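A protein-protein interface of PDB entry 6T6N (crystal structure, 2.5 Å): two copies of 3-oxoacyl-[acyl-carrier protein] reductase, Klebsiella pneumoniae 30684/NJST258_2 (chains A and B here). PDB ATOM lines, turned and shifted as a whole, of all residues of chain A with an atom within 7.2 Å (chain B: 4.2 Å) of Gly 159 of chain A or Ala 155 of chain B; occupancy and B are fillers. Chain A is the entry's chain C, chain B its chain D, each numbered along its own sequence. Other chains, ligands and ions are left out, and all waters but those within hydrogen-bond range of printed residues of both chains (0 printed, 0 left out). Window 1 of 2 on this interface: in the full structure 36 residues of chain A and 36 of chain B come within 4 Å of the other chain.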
ATOM      1  N   ASN A 113      -1.258 -14.113  25.385  1.00  0.00           N
ATOM      2  CA  ASN A 113      -1.237 -13.459  24.072  1.00  0.00           C
ATOM      3  C   ASN A 113      -0.098 -13.929  23.196  1.00  0.00           C
ATOM      4  O   ASN A 113      -0.267 -14.069  21.982  1.00  0.00           O
ATOM      5  CB  ASN A 113      -1.119 -11.939  24.223  1.00  0.00           C
ATOM      6  CG  ASN A 113      -2.337 -11.315  24.888  1.00  0.00           C
ATOM      7  OD1 ASN A 113      -3.259 -12.003  25.322  1.00  0.00           O
ATOM      8  ND2 ASN A 113      -2.337  -9.997  24.981  1.00  0.00           N
ATOM      9  N   LEU A 114       1.069 -14.129  23.799  1.00  0.00           N
ATOM     10  CA  LEU A 114       2.262 -14.432  23.034  1.00  0.00           C
ATOM     11  C   LEU A 114       2.518 -15.941  23.015  1.00  0.00           C
ATOM     12  O   LEU A 114       2.481 -16.562  21.948  1.00  0.00           O
ATOM     13  CB  LEU A 114       3.467 -13.655  23.558  1.00  0.00           C
ATOM     14  CG  LEU A 114       4.716 -13.731  22.686  1.00  0.00           C
ATOM     15  CD1 LEU A 114       4.472 -13.278  21.248  1.00  0.00           C
ATOM     16  CD2 LEU A 114       5.848 -12.954  23.340  1.00  0.00           C
ATOM     17  N   PHE A 118       1.753 -18.780  20.116  1.00  0.00           N
ATOM     18  CA  PHE A 118       2.827 -19.664  19.658  1.00  0.00           C
ATOM     19  C   PHE A 118       2.418 -21.151  19.697  1.00  0.00           C
ATOM     20  O   PHE A 118       2.608 -21.879  18.726  1.00  0.00           O
ATOM     21  CB  PHE A 118       4.116 -19.457  20.478  1.00  0.00           C
ATOM     22  CG  PHE A 118       5.012 -20.665  20.528  1.00  0.00           C
ATOM     23  CD1 PHE A 118       5.566 -21.168  19.365  1.00  0.00           C
ATOM     24  CD2 PHE A 118       5.282 -21.303  21.736  1.00  0.00           C
ATOM     25  CE1 PHE A 118       6.375 -22.300  19.388  1.00  0.00           C
ATOM     26  CE2 PHE A 118       6.092 -22.434  21.769  1.00  0.00           C
ATOM     27  CZ  PHE A 118       6.657 -22.922  20.589  1.00  0.00           C
ATOM     28  N   MET A 121      -0.094 -21.891  16.934  1.00  0.00           N
ATOM     29  CA  MET A 121       0.619 -21.816  15.656  1.00  0.00           C
ATOM     30  C   MET A 121       1.459 -23.082  15.414  1.00  0.00           C
ATOM     31  O   MET A 121       1.500 -23.607  14.296  1.00  0.00           O
ATOM     32  CB  MET A 121       1.540 -20.601  15.616  1.00  0.00           C
ATOM     33  CG  MET A 121       0.854 -19.273  15.341  1.00  0.00           C
ATOM     34  SD  MET A 121       2.023 -17.892  15.362  1.00  0.00           S
ATOM     35  CE  MET A 121       2.915 -18.205  13.849  1.00  0.00           C
ATOM     36  N   TRP A 144       0.622  -2.662  18.728  1.00  0.00           N
ATOM     37  CA  TRP A 144       1.940  -3.300  18.517  1.00  0.00           C
ATOM     38  C   TRP A 144       3.059  -2.305  18.266  1.00  0.00           C
ATOM     39  O   TRP A 144       4.213  -2.613  18.550  1.00  0.00           O
ATOM     40  CB  TRP A 144       1.893  -4.381  17.427  1.00  0.00           C
ATOM     41  CG  TRP A 144       1.970  -3.934  15.979  1.00  0.00           C
ATOM     42  CD1 TRP A 144       0.991  -3.342  15.255  1.00  0.00           C
ATOM     43  CD2 TRP A 144       3.065  -4.120  15.082  1.00  0.00           C
ATOM     44  NE1 TRP A 144       1.406  -3.116  13.980  1.00  0.00           N
ATOM     45  CE2 TRP A 144       2.677  -3.593  13.837  1.00  0.00           C
ATOM     46  CE3 TRP A 144       4.337  -4.676  15.205  1.00  0.00           C
ATOM     47  CZ2 TRP A 144       3.521  -3.596  12.714  1.00  0.00           C
ATOM     48  CZ3 TRP A 144       5.180  -4.688  14.085  1.00  0.00           C
ATOM     49  CH2 TRP A 144       4.756  -4.150  12.859  1.00  0.00           C
ATOM     50  N   TYR A 153       1.006  -5.556  26.885  1.00  0.00           N
ATOM     51  CA  TYR A 153       0.139  -5.853  25.748  1.00  0.00           C
ATOM     52  C   TYR A 153       0.844  -5.573  24.414  1.00  0.00           C
ATOM     53  O   TYR A 153       0.798  -6.402  23.508  1.00  0.00           O
ATOM     54  CB  TYR A 153      -1.143  -5.042  25.860  1.00  0.00           C
ATOM     55  CG  TYR A 153      -2.215  -5.353  24.851  1.00  0.00           C
ATOM     56  CD1 TYR A 153      -2.966  -6.530  24.940  1.00  0.00           C
ATOM     57  CD2 TYR A 153      -2.519  -4.449  23.839  1.00  0.00           C
ATOM     58  CE1 TYR A 153      -3.978  -6.800  24.020  1.00  0.00           C
ATOM     59  CE2 TYR A 153      -3.520  -4.705  22.924  1.00  0.00           C
ATOM     60  CZ  TYR A 153      -4.254  -5.880  23.006  1.00  0.00           C
ATOM     61  OH  TYR A 153      -5.240  -6.115  22.068  1.00  0.00           O
ATOM     62  N   SER A 154       1.496  -4.417  24.307  1.00  0.00           N
ATOM     63  CA  SER A 154       2.217  -4.056  23.094  1.00  0.00           C
ATOM     64  C   SER A 154       3.370  -5.034  22.827  1.00  0.00           C
ATOM     65  O   SER A 154       3.585  -5.447  21.695  1.00  0.00           O
ATOM     66  CB  SER A 154       2.727  -2.610  23.146  1.00  0.00           C
ATOM     67  OG  SER A 154       3.736  -2.442  24.129  1.00  0.00           O
ATOM     68  N   ALA A 155       4.081  -5.421  23.873  1.00  0.00           N
ATOM     69  CA  ALA A 155       5.127  -6.434  23.745  1.00  0.00           C
ATOM     70  C   ALA A 155       4.559  -7.705  23.156  1.00  0.00           C
ATOM     71  O   ALA A 155       5.123  -8.276  22.229  1.00  0.00           O
ATOM     72  CB  ALA A 155       5.724  -6.748  25.098  1.00  0.00           C
ATOM     73  N   SER A 156       3.429  -8.134  23.702  1.00  0.00           N
ATOM     74  CA  SER A 156       2.831  -9.399  23.314  1.00  0.00           C
ATOM     75  C   SER A 156       2.351  -9.377  21.874  1.00  0.00           C
ATOM     76  O   SER A 156       2.545 -10.341  21.154  1.00  0.00           O
ATOM     77  CB  SER A 156       1.676  -9.773  24.259  1.00  0.00           C
ATOM     78  OG  SER A 156       0.509  -9.016  24.000  1.00  0.00           O
ATOM     79  N   LYS A 157       1.739  -8.270  21.463  1.00  0.00           N
ATOM     80  CA  LYS A 157       1.162  -8.169  20.131  1.00  0.00           C
ATOM     81  C   LYS A 157       2.205  -7.914  19.040  1.00  0.00           C
ATOM     82  O   LYS A 157       2.064  -8.427  17.938  1.00  0.00           O
ATOM     83  CB  LYS A 157       0.066  -7.109  20.097  1.00  0.00           C
ATOM     84  CG  LYS A 157      -1.143  -7.440  20.969  1.00  0.00           C
ATOM     85  CD  LYS A 157      -1.814  -8.770  20.608  1.00  0.00           C
ATOM     86  CE  LYS A 157      -3.229  -8.818  21.128  1.00  0.00           C
ATOM     87  NZ  LYS A 157      -4.032  -9.927  20.575  1.00  0.00           N
ATOM     88  N   ALA A 158       3.234  -7.124  19.337  1.00  0.00           N
ATOM     89  CA  ALA A 158       4.381  -6.996  18.437  1.00  0.00           C
ATOM     90  C   ALA A 158       5.063  -8.353  18.268  1.00  0.00           C
ATOM     91  O   ALA A 158       5.423  -8.748  17.157  1.00  0.00           O
ATOM     92  CB  ALA A 158       5.371  -5.965  18.964  1.00  0.00           C
ATOM     93  N   GLY A 159       5.202  -9.070  19.371  1.00  0.00           N
ATOM     94  CA  GLY A 159       5.692 -10.444  19.340  1.00  0.00           C
ATOM     95  C   GLY A 159       4.906 -11.316  18.382  1.00  0.00           C
ATOM     96  O   GLY A 159       5.479 -12.070  17.609  1.00  0.00           O
ATOM     97  N   VAL A 160       3.590 -11.202  18.422  1.00  0.00           N
ATOM     98  CA  VAL A 160       2.753 -11.948  17.503  1.00  0.00           C
ATOM     99  C   VAL A 160       3.066 -11.592  16.055  1.00  0.00           C
ATOM    100  O   VAL A 160       3.102 -12.479  15.198  1.00  0.00           O
ATOM    101  CB  VAL A 160       1.263 -11.780  17.844  1.00  0.00           C
ATOM    102  CG1 VAL A 160       0.359 -12.249  16.713  1.00  0.00           C
ATOM    103  CG2 VAL A 160       0.942 -12.555  19.127  1.00  0.00           C
ATOM    104  N   VAL A 161       3.315 -10.317  15.772  1.00  0.00           N
ATOM    105  CA  VAL A 161       3.672  -9.905  14.411  1.00  0.00           C
ATOM    106  C   VAL A 161       4.996 -10.548  13.985  1.00  0.00           C
ATOM    107  O   VAL A 161       5.110 -11.046  12.878  1.00  0.00           O
ATOM    108  CB  VAL A 161       3.704  -8.372  14.256  1.00  0.00           C
ATOM    109  CG1 VAL A 161       4.254  -7.963  12.889  1.00  0.00           C
ATOM    110  CG2 VAL A 161       2.300  -7.801  14.431  1.00  0.00           C
ATOM    111  N   GLY A 162       5.988 -10.530  14.862  1.00  0.00           N
ATOM    112  CA  GLY A 162       7.272 -11.178  14.588  1.00  0.00           C
ATOM    113  C   GLY A 162       7.145 -12.664  14.245  1.00  0.00           C
ATOM    114  O   GLY A 162       7.721 -13.127  13.256  1.00  0.00           O
ATOM    115  N   MET A 163       6.377 -13.399  15.048  1.00  0.00           N
ATOM    116  CA  MET A 163       6.137 -14.834  14.814  1.00  0.00           C
ATOM    117  C   MET A 163       5.415 -15.079  13.509  1.00  0.00           C
ATOM    118  O   MET A 163       5.715 -16.038  12.809  1.00  0.00           O
ATOM    119  CB  MET A 163       5.298 -15.454  15.930  1.00  0.00           C
ATOM    120  CG  MET A 163       5.987 -15.489  17.271  1.00  0.00           C
ATOM    121  SD  MET A 163       5.150 -16.496  18.499  1.00  0.00           S
ATOM    122  CE  MET A 163       3.471 -15.838  18.499  1.00  0.00           C
ATOM    123  N   THR A 164       4.448 -14.218  13.213  1.00  0.00           N
ATOM    124  CA  THR A 164       3.700 -14.261  11.966  1.00  0.00           C
ATOM    125  C   THR A 164       4.636 -14.229  10.777  1.00  0.00           C
ATOM    126  O   THR A 164       4.528 -15.032   9.862  1.00  0.00           O
ATOM    127  CB  THR A 164       2.716 -13.076  11.885  1.00  0.00           C
ATOM    128  OG1 THR A 164       1.826 -13.114  13.009  1.00  0.00           O
ATOM    129  CG2 THR A 164       1.894 -13.082  10.617  1.00  0.00           C
ATOM    130  N   LYS A 165       5.562 -13.292  10.796  1.00  0.00           N
ATOM    131  CA  LYS A 165       6.495 -13.126   9.687  1.00  0.00           C
ATOM    132  C   LYS A 165       7.513 -14.266   9.610  1.00  0.00           C
ATOM    133  O   LYS A 165       7.870 -14.715   8.512  1.00  0.00           O
ATOM    134  CB  LYS A 165       7.177 -11.774   9.784  1.00  0.00           C
ATOM    135  CG  LYS A 165       6.230 -10.654   9.443  1.00  0.00           C
ATOM    136  CD  LYS A 165       6.874  -9.294   9.672  1.00  0.00           C
ATOM    137  CE  LYS A 165       5.907  -8.181   9.306  1.00  0.00           C
ATOM    138  NZ  LYS A 165       5.647  -8.134   7.838  1.00  0.00           N
ATOM    139  N   THR A 166       7.974 -14.723  10.767  1.00  0.00           N
ATOM    140  CA  THR A 166       8.827 -15.893  10.838  1.00  0.00           C
ATOM    141  C   THR A 166       8.127 -17.130  10.232  1.00  0.00           C
ATOM    142  O   THR A 166       8.707 -17.835   9.397  1.00  0.00           O
ATOM    143  CB  THR A 166       9.242 -16.175  12.284  1.00  0.00           C
ATOM    144  OG1 THR A 166      10.175 -15.174  12.697  1.00  0.00           O
ATOM    145  CG2 THR A 166       9.884 -17.570  12.428  1.00  0.00           C
ATOM    146  N   TRP B 106      11.478 -21.912  24.073  1.00  0.00           N
ATOM    147  CA  TRP B 106      10.584 -20.767  23.980  1.00  0.00           C
ATOM    148  C   TRP B 106      10.693 -19.956  25.272  1.00  0.00           C
ATOM    149  O   TRP B 106      11.028 -18.778  25.237  1.00  0.00           O
ATOM    150  CB  TRP B 106       9.115 -21.186  23.744  1.00  0.00           C
ATOM    151  CG  TRP B 106       8.177 -20.049  24.006  1.00  0.00           C
ATOM    152  CD1 TRP B 106       7.621 -19.713  25.195  1.00  0.00           C
ATOM    153  CD2 TRP B 106       7.751 -19.068  23.068  1.00  0.00           C
ATOM    154  NE1 TRP B 106       6.866 -18.581  25.062  1.00  0.00           N
ATOM    155  CE2 TRP B 106       6.924 -18.164  23.762  1.00  0.00           C
ATOM    156  CE3 TRP B 106       7.980 -18.867  21.700  1.00  0.00           C
ATOM    157  CZ2 TRP B 106       6.335 -17.064  23.148  1.00  0.00           C
ATOM    158  CZ3 TRP B 106       7.395 -17.770  21.082  1.00  0.00           C
ATOM    159  CH2 TRP B 106       6.573 -16.883  21.809  1.00  0.00           C
ATOM    160  N   THR B 151      11.230 -18.269  15.675  1.00  0.00           N
ATOM    161  CA  THR B 151       9.926 -17.954  16.235  1.00  0.00           C
ATOM    162  C   THR B 151      10.063 -17.281  17.618  1.00  0.00           C
ATOM    163  O   THR B 151       9.486 -16.221  17.856  1.00  0.00           O
ATOM    164  CB  THR B 151       9.049 -19.208  16.313  1.00  0.00           C
ATOM    165  OG1 THR B 151       8.698 -19.590  14.980  1.00  0.00           O
ATOM    166  CG2 THR B 151       7.766 -18.950  17.089  1.00  0.00           C
ATOM    167  N   ASN B 152      10.839 -17.887  18.506  1.00  0.00           N
ATOM    168  CA  ASN B 152      11.012 -17.332  19.845  1.00  0.00           C
ATOM    169  C   ASN B 152      11.813 -16.014  19.847  1.00  0.00           C
ATOM    170  O   ASN B 152      11.423 -15.045  20.507  1.00  0.00           O
ATOM    171  CB  ASN B 152      11.614 -18.345  20.830  1.00  0.00           C
ATOM    172  CG  ASN B 152      12.917 -18.974  20.349  1.00  0.00           C
ATOM    173  OD1 ASN B 152      13.346 -18.816  19.199  1.00  0.00           O
ATOM    174  ND2 ASN B 152      13.546 -19.721  21.246  1.00  0.00           N
ATOM    175  N   TYR B 153      12.900 -15.978  19.087  1.00  0.00           N
ATOM    176  CA  TYR B 153      13.772 -14.803  19.060  1.00  0.00           C
ATOM    177  C   TYR B 153      13.076 -13.598  18.419  1.00  0.00           C
ATOM    178  O   TYR B 153      13.120 -12.501  18.964  1.00  0.00           O
ATOM    179  CB  TYR B 153      15.063 -15.129  18.324  1.00  0.00           C
ATOM    180  CG  TYR B 153      16.136 -14.078  18.346  1.00  0.00           C
ATOM    181  CD1 TYR B 153      16.886 -13.848  19.486  1.00  0.00           C
ATOM    182  CD2 TYR B 153      16.446 -13.354  17.205  1.00  0.00           C
ATOM    183  CE1 TYR B 153      17.910 -12.878  19.491  1.00  0.00           C
ATOM    184  CE2 TYR B 153      17.464 -12.416  17.194  1.00  0.00           C
ATOM    185  CZ  TYR B 153      18.189 -12.176  18.340  1.00  0.00           C
ATOM    186  OH  TYR B 153      19.193 -11.225  18.313  1.00  0.00           O
ATOM    187  N   SER B 154      12.427 -13.817  17.278  1.00  0.00           N
ATOM    188  CA  SER B 154      11.707 -12.744  16.588  1.00  0.00           C
ATOM    189  C   SER B 154      10.556 -12.218  17.453  1.00  0.00           C
ATOM    190  O   SER B 154      10.350 -11.013  17.532  1.00  0.00           O
ATOM    191  CB  SER B 154      11.198 -13.199  15.214  1.00  0.00           C
ATOM    192  OG  SER B 154      10.195 -14.188  15.324  1.00  0.00           O
ATOM    193  N   ALA B 155       9.838 -13.114  18.113  1.00  0.00           N
ATOM    194  CA  ALA B 155       8.795 -12.708  19.047  1.00  0.00           C
ATOM    195  C   ALA B 155       9.361 -11.780  20.102  1.00  0.00           C
ATOM    196  O   ALA B 155       8.797 -10.728  20.393  1.00  0.00           O
ATOM    197  CB  ALA B 155       8.187 -13.921  19.733  1.00  0.00           C
ATOM    198  N   SER B 156      10.485 -12.194  20.672  1.00  0.00           N
ATOM    199  CA  SER B 156      11.079 -11.473  21.778  1.00  0.00           C
ATOM    200  C   SER B 156      11.573 -10.089  21.355  1.00  0.00           C
ATOM    201  O   SER B 156      11.380  -9.126  22.084  1.00  0.00           O
ATOM    202  CB  SER B 156      12.217 -12.278  22.406  1.00  0.00           C
ATOM    203  OG  SER B 156      13.398 -12.240  21.602  1.00  0.00           O
ATOM    204  N   LYS B 157      12.189 -10.010  20.184  1.00  0.00           N
ATOM    205  CA  LYS B 157      12.772  -8.761  19.715  1.00  0.00           C
ATOM    206  C   LYS B 157      11.743  -7.779  19.156  1.00  0.00           C
ATOM    207  O   LYS B 157      11.890  -6.584  19.344  1.00  0.00           O
ATOM    208  CB  LYS B 157      13.874  -9.037  18.682  1.00  0.00           C
ATOM    209  CG  LYS B 157      15.078  -9.782  19.261  1.00  0.00           C
ATOM    210  CD  LYS B 157      15.746  -9.052  20.418  1.00  0.00           C
ATOM    211  CE  LYS B 157      17.179  -9.526  20.615  1.00  0.00           C
ATOM    212  NZ  LYS B 157      17.936  -8.678  21.564  1.00  0.00           N
ATOM    213  N   ALA B 158      10.712  -8.282  18.481  1.00  0.00           N
ATOM    214  CA  ALA B 158       9.567  -7.450  18.102  1.00  0.00           C
ATOM    215  C   ALA B 158       8.891  -6.902  19.357  1.00  0.00           C
ATOM    216  O   ALA B 158       8.531  -5.726  19.424  1.00  0.00           O
ATOM    217  CB  ALA B 158       8.576  -8.240  17.259  1.00  0.00           C
ATOM    218  N   GLY B 159       8.748  -7.753  20.356  1.00  0.00           N
ATOM    219  CA  GLY B 159       8.250  -7.333  21.659  1.00  0.00           C
ATOM    220  C   GLY B 159       9.041  -6.172  22.229  1.00  0.00           C
ATOM    221  O   GLY B 159       8.468  -5.216  22.734  1.00  0.00           O
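O of Gly 162 of chain A sits at hydrogen-bond distance from OG of Ser 154 of chain B (3.4 Å).
The side-chain hydroxyl (OG1) of Thr 166 of chain A is in hydrogen-bond range of the side-chain hydroxyl (OG) of Ser 154 of chain B.
OG1 of Thr 166 of chain A is in hydrogen-bond range of O of Gly 162 of chain A, 3.2 Å away.
O of Thr 151 of chain B sits at hydrogen-bond distance from OG of Ser 154 of chain B, 3.3 Å away.
CG2 of Thr 151 of chain B touches CD1 of Phe 118 of chain A (3.9 Å).
CA of Gly 159 of chain B touches O of Ala 155 of chain A, 3.3 Å away.
Ala 158 of chain B touches Ala 158 of chain A (CB to O, 3.2 Å).
O of Ala 155 of chain B touches CA of Gly 159 of chain A, 3.3 Å away.
Gly 159 of chain A touches Gly 159 of chain B.
Met 163 of chain A touches Trp 106 of chain B (SD to CH2, 3.6 Å).
CG of Met 163 of chain A touches O of Thr 151 of chain B, at 3.6 Å.
Ser 154 of chain B touches Met 163 of chain A.
Ala 155 of chain B touches Met 163 of chain A (CB to CG, 3.7 Å).
Thr 151 of chain B touches Thr 166 of chain A.
Gly 159 of chain A touches two residues of chain B.
Of chain A, only Gly 159 and Met 163 come within 4 Å of Ala 155 of chain B.
Printed residues of chain B within 4 Å of Met 163 of chain A: Trp 106, Thr 151, Ser 154 and Ala 155.
Of the printed residues of chain A, Gly 159 of chain B touches Ala 155 and Gly 159.
Lys 157 of chain A touches none of the printed residues of chain B.
Hydrophobic or aromatic side chains of chain B within 4 Å of the printed part of chain A: Trp 106, Ala 155 and Ala 158.
Hydrophobic or aromatic side chains of chain A within 4 Å of the printed part of chain B: Leu 114, Phe 118, Ala 155, Ala 158 and Met 163.
Among the printed residues, 14 pairs touch across the chains.
Ala 155 of chain A touches Gly 159 of chain B, and with the chains exchanged Gly 159 of chain A touches Ala 155 of chain B.
Ala 158 of chain A touches its own counterpart, Ala 158 of chain B.
Gly 159 of chain A touches its own counterpart, Gly 159 of chain B.
Positions printed for both chains: 153, 154, 155, 156, 157, 158 and 159.
Of the 14 pairs that touch across the chains among the printed residues, 4 have their exchanged pair printed and touching as well.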
